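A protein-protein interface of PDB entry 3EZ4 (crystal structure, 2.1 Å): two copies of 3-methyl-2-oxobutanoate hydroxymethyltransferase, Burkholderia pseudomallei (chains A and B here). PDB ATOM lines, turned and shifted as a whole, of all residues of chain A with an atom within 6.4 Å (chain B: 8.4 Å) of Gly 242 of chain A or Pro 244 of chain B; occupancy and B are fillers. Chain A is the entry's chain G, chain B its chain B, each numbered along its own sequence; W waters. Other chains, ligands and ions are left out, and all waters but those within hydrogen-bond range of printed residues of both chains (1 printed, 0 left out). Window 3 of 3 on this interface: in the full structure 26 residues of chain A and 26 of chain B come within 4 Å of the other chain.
Among the printed residues, pairs that only touch across the chains: Met 240 of chain A with Met 240 of chain B (2.9 Å), Pro 244 of chain A with Gln 241 of chain B (3.6 Å), Gln 241 of chain A with Ser 245 of chain B (3.6 Å), Gly 242 of chain A with Pro 244 of chain B (3.6 Å) and Gln 243 of chain A with Gln 243 of chain B (3.7 Å).
The backbone NH (N) of Phe 247 of chain B lies close to the side-chain hydroxyl (OG) of Ser 245 of chain B.
The side-chain hydroxyl (OG) of Ser 245 of chain B lies within hydrogen-bond range of the backbone NH (N) of Ala 248 of chain B (3.1 Å).
Of the printed residues of chain B, Met 240 of chain A touches Met 240.
Of chain B, only Pro 244 comes within 4 Å of Gly 242 of chain A.
Printed residues of chain A within 4 Å of Gln 243 of chain B: Gln 243 (3.7 Å).
Of chain A, only Gln 241 and Gly 242 come within 4 Å of Pro 244 of chain B.
Water W1 lies within hydrogen-bond range of O of Gln 243 of chain B and O of Gln 243 of chain A.
Of the 12 printed residues of chain B, 6 touch a printed residue of chain A.
Hydrophobic or aromatic side chains of chain B that line the printed part of chain A: Met 240.
Among the printed residues, no Asp or Glu carboxylate lies within 4 Å of a Lys or Arg side-chain nitrogen of the other chain.
Met 240 of chain A touches its own counterpart, Met 240 of chain B.
Gln 241 of chain A touches Pro 244 of chain B, and with the chains exchanged Pro 244 of chain A touches Gln 241 of chain B.
Gly 242 of chain A touches Pro 244 of chain B, and with the chains exchanged Pro 244 of chain A touches Gly 242 of chain B.
Gln 243 of chain A touches its own counterpart, Gln 243 of chain B.
Positions printed for both chains: 239, 240, 241, 242, 243 and 244.
OE1 of Gln 241 of chain A sits close to O of Pro 244 of chain B (3.0 Å).
O of Pro 244 of chain A is in hydrogen-bond range of N of Gly 242 of chain B (3.3 Å).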
ATOM      1  N   PHE A 239      19.398  31.130   8.932  1.00  0.00           N
ATOM      2  CA  PHE A 239      19.500  31.518   7.537  1.00  0.00           C
ATOM      3  C   PHE A 239      20.667  30.877   6.807  1.00  0.00           C
ATOM      4  O   PHE A 239      20.770  31.003   5.575  1.00  0.00           O
ATOM      5  CB  PHE A 239      19.461  33.043   7.352  1.00  0.00           C
ATOM      6  CG  PHE A 239      18.077  33.591   7.422  1.00  0.00           C
ATOM      7  CD1 PHE A 239      17.281  33.655   6.269  1.00  0.00           C
ATOM      8  CD2 PHE A 239      17.514  33.969   8.642  1.00  0.00           C
ATOM      9  CE1 PHE A 239      15.950  34.130   6.344  1.00  0.00           C
ATOM     10  CE2 PHE A 239      16.214  34.430   8.719  1.00  0.00           C
ATOM     11  CZ  PHE A 239      15.421  34.513   7.556  1.00  0.00           C
ATOM     12  N   MET A 240      21.526  30.162   7.529  1.00  0.00           N
ATOM     13  CA  MET A 240      22.773  29.649   6.915  1.00  0.00           C
ATOM     14  C   MET A 240      22.480  28.297   6.253  1.00  0.00           C
ATOM     15  O   MET A 240      22.847  28.051   5.117  1.00  0.00           O
ATOM     16  CB  MET A 240      23.885  29.568   8.002  1.00  0.00           C
ATOM     17  CG  MET A 240      25.222  29.106   7.548  1.00  0.00           C
ATOM     18  SD  MET A 240      26.008  30.223   6.404  1.00  0.00           S
ATOM     19  CE  MET A 240      26.485  28.984   5.188  1.00  0.00           C
ATOM     20  N   GLN A 241      21.755  27.449   6.964  1.00  0.00           N
ATOM     21  CA  GLN A 241      21.458  26.096   6.504  1.00  0.00           C
ATOM     22  C   GLN A 241      21.003  26.125   5.048  1.00  0.00           C
ATOM     23  O   GLN A 241      20.038  26.808   4.707  1.00  0.00           O
ATOM     24  CB  GLN A 241      20.414  25.430   7.436  1.00  0.00           C
ATOM     25  CG  GLN A 241      20.404  23.882   7.443  1.00  0.00           C
ATOM     26  CD  GLN A 241      21.670  23.252   8.051  1.00  0.00           C
ATOM     27  OE1 GLN A 241      22.660  23.943   8.304  1.00  0.00           O
ATOM     28  NE2 GLN A 241      21.642  21.940   8.268  1.00  0.00           N
ATOM     29  N   GLY A 242      21.740  25.422   4.186  1.00  0.00           N
ATOM     30  CA  GLY A 242      21.377  25.332   2.754  1.00  0.00           C
ATOM     31  C   GLY A 242      21.836  26.480   1.859  1.00  0.00           C
ATOM     32  O   GLY A 242      21.473  26.532   0.671  1.00  0.00           O
ATOM     33  N   GLN A 243      22.607  27.425   2.404  1.00  0.00           N
ATOM     34  CA  GLN A 243      23.130  28.567   1.603  1.00  0.00           C
ATOM     35  C   GLN A 243      24.568  28.323   1.290  1.00  0.00           C
ATOM     36  O   GLN A 243      25.226  27.617   2.008  1.00  0.00           O
ATOM     37  CB  GLN A 243      23.029  29.898   2.366  1.00  0.00           C
ATOM     38  CG  GLN A 243      21.630  30.356   2.623  1.00  0.00           C
ATOM     39  CD  GLN A 243      20.897  30.777   1.376  1.00  0.00           C
ATOM     40  OE1 GLN A 243      21.488  31.058   0.339  1.00  0.00           O
ATOM     41  NE2 GLN A 243      19.599  30.834   1.478  1.00  0.00           N
ATOM     42  N   PRO A 244      25.068  28.889   0.185  1.00  0.00           N
ATOM     43  CA  PRO A 244      26.434  28.538  -0.187  1.00  0.00           C
ATOM     44  C   PRO A 244      27.541  29.305   0.572  1.00  0.00           C
ATOM     45  O   PRO A 244      28.693  28.894   0.496  1.00  0.00           O
ATOM     46  CB  PRO A 244      26.483  28.905  -1.659  1.00  0.00           C
ATOM     47  CG  PRO A 244      25.512  29.984  -1.798  1.00  0.00           C
ATOM     48  CD  PRO A 244      24.420  29.735  -0.828  1.00  0.00           C
ATOM     49  N   PHE B 239      37.064  26.975   3.456  1.00  0.00           N
ATOM     50  CA  PHE B 239      36.347  25.736   3.723  1.00  0.00           C
ATOM     51  C   PHE B 239      34.829  25.900   3.880  1.00  0.00           C
ATOM     52  O   PHE B 239      34.128  24.919   4.077  1.00  0.00           O
ATOM     53  CB  PHE B 239      36.910  25.062   4.964  1.00  0.00           C
ATOM     54  CG  PHE B 239      38.203  24.377   4.732  1.00  0.00           C
ATOM     55  CD1 PHE B 239      38.228  23.043   4.347  1.00  0.00           C
ATOM     56  CD2 PHE B 239      39.409  25.058   4.903  1.00  0.00           C
ATOM     57  CE1 PHE B 239      39.429  22.413   4.121  1.00  0.00           C
ATOM     58  CE2 PHE B 239      40.593  24.437   4.685  1.00  0.00           C
ATOM     59  CZ  PHE B 239      40.612  23.102   4.292  1.00  0.00           C
ATOM     60  N   MET B 240      34.317  27.128   3.839  1.00  0.00           N
ATOM     61  CA  MET B 240      32.881  27.347   4.008  1.00  0.00           C
ATOM     62  C   MET B 240      32.185  27.076   2.680  1.00  0.00           C
ATOM     63  O   MET B 240      31.126  26.501   2.662  1.00  0.00           O
ATOM     64  CB  MET B 240      32.587  28.774   4.486  1.00  0.00           C
ATOM     65  CG  MET B 240      31.119  29.058   4.801  1.00  0.00           C
ATOM     66  SD  MET B 240      30.469  27.985   6.084  1.00  0.00           S
ATOM     67  CE  MET B 240      28.936  27.397   5.384  1.00  0.00           C
ATOM     68  N   GLN B 241      32.813  27.461   1.572  1.00  0.00           N
ATOM     69  CA  GLN B 241      32.127  27.481   0.284  1.00  0.00           C
ATOM     70  C   GLN B 241      31.576  26.101  -0.044  1.00  0.00           C
ATOM     71  O   GLN B 241      32.310  25.119  -0.108  1.00  0.00           O
ATOM     72  CB  GLN B 241      33.038  27.993  -0.827  1.00  0.00           C
ATOM     73  CG  GLN B 241      32.247  28.441  -2.092  1.00  0.00           C
ATOM     74  CD  GLN B 241      31.331  29.669  -1.881  1.00  0.00           C
ATOM     75  OE1 GLN B 241      31.627  30.573  -1.075  1.00  0.00           O
ATOM     76  NE2 GLN B 241      30.207  29.702  -2.625  1.00  0.00           N
ATOM     77  N   GLY B 242      30.249  26.042  -0.166  1.00  0.00           N
ATOM     78  CA  GLY B 242      29.546  24.807  -0.522  1.00  0.00           C
ATOM     79  C   GLY B 242      29.376  23.789   0.586  1.00  0.00           C
ATOM     80  O   GLY B 242      29.131  22.610   0.315  1.00  0.00           O
ATOM     81  N   GLN B 243      29.505  24.211   1.839  1.00  0.00           N
ATOM     82  CA  GLN B 243      29.214  23.333   2.955  1.00  0.00           C
ATOM     83  C   GLN B 243      27.854  23.710   3.450  1.00  0.00           C
ATOM     84  O   GLN B 243      27.413  24.825   3.215  1.00  0.00           O
ATOM     85  CB  GLN B 243      30.233  23.551   4.062  1.00  0.00           C
ATOM     86  CG  GLN B 243      31.612  23.141   3.647  1.00  0.00           C
ATOM     87  CD  GLN B 243      31.750  21.636   3.585  1.00  0.00           C
ATOM     88  OE1 GLN B 243      30.931  20.899   4.163  1.00  0.00           O
ATOM     89  NE2 GLN B 243      32.791  21.166   2.904  1.00  0.00           N
ATOM     90  N   PRO B 244      27.187  22.791   4.149  1.00  0.00           N
ATOM     91  CA  PRO B 244      25.837  23.023   4.590  1.00  0.00           C
ATOM     92  C   PRO B 244      25.714  23.879   5.858  1.00  0.00           C
ATOM     93  O   PRO B 244      24.623  24.400   6.148  1.00  0.00           O
ATOM     94  CB  PRO B 244      25.329  21.605   4.872  1.00  0.00           C
ATOM     95  CG  PRO B 244      26.473  20.820   5.108  1.00  0.00           C
ATOM     96  CD  PRO B 244      27.556  21.370   4.264  1.00  0.00           C
ATOM     97  N   SER B 245      26.817  24.046   6.600  1.00  0.00           N
ATOM     98  CA  SER B 245      26.786  24.819   7.823  1.00  0.00           C
ATOM     99  C   SER B 245      28.212  25.255   8.181  1.00  0.00           C
ATOM    100  O   SER B 245      29.193  24.699   7.659  1.00  0.00           O
ATOM    101  CB  SER B 245      26.178  23.954   8.932  1.00  0.00           C
ATOM    102  OG  SER B 245      27.107  22.949   9.336  1.00  0.00           O
ATOM    103  N   ILE B 246      28.322  26.222   9.093  1.00  0.00           N
ATOM    104  CA  ILE B 246      29.645  26.641   9.605  1.00  0.00           C
ATOM    105  C   ILE B 246      30.316  25.459  10.327  1.00  0.00           C
ATOM    106  O   ILE B 246      31.484  25.227  10.154  1.00  0.00           O
ATOM    107  CB  ILE B 246      29.526  27.906  10.520  1.00  0.00           C
ATOM    108  CG1 ILE B 246      28.999  29.095   9.688  1.00  0.00           C
ATOM    109  CG2 ILE B 246      30.869  28.234  11.188  1.00  0.00           C
ATOM    110  CD1 ILE B 246      28.622  30.390  10.518  1.00  0.00           C
ATOM    111  N   PHE B 247      29.565  24.697  11.110  1.00  0.00           N
ATOM    112  CA  PHE B 247      30.122  23.516  11.742  1.00  0.00           C
ATOM    113  C   PHE B 247      30.742  22.551  10.679  1.00  0.00           C
ATOM    114  O   PHE B 247      31.807  21.965  10.955  1.00  0.00           O
ATOM    115  CB  PHE B 247      29.063  22.794  12.579  1.00  0.00           C
ATOM    116  CG  PHE B 247      29.518  21.479  13.142  1.00  0.00           C
ATOM    117  CD1 PHE B 247      30.354  21.427  14.238  1.00  0.00           C
ATOM    118  CD2 PHE B 247      29.087  20.267  12.568  1.00  0.00           C
ATOM    119  CE1 PHE B 247      30.756  20.209  14.762  1.00  0.00           C
ATOM    120  CE2 PHE B 247      29.508  19.053  13.069  1.00  0.00           C
ATOM    121  CZ  PHE B 247      30.330  19.026  14.194  1.00  0.00           C
ATOM    122  N   ALA B 248      30.107  22.393   9.494  1.00  0.00           N
ATOM    123  CA  ALA B 248      30.626  21.434   8.504  1.00  0.00           C
ATOM    124  C   ALA B 248      31.868  22.008   7.874  1.00  0.00           C
ATOM    125  O   ALA B 248      32.810  21.264   7.579  1.00  0.00           O
ATOM    126  CB  ALA B 248      29.583  21.061   7.422  1.00  0.00           C
ATOM    127  N   ALA B 249      31.918  23.335   7.718  1.00  0.00           N
ATOM    128  CA  ALA B 249      33.158  23.991   7.252  1.00  0.00           C
ATOM    129  C   ALA B 249      34.364  23.649   8.151  1.00  0.00           C
ATOM    130  O   ALA B 249      35.423  23.297   7.651  1.00  0.00           O
ATOM    131  CB  ALA B 249      32.984  25.462   7.114  1.00  0.00           C
ATOM    132  N   ALA B 252      35.367  20.127   8.069  1.00  0.00           N
ATOM    133  CA  ALA B 252      36.058  19.812   6.830  1.00  0.00           C
ATOM    134  C   ALA B 252      37.528  20.245   6.918  1.00  0.00           C
ATOM    135  O   ALA B 252      38.453  19.547   6.414  1.00  0.00           O
ATOM    136  CB  ALA B 252      35.375  20.446   5.651  1.00  0.00           C
HETATM  137  O   HOH W   1      25.247  24.786   1.318  1.00  0.00           O
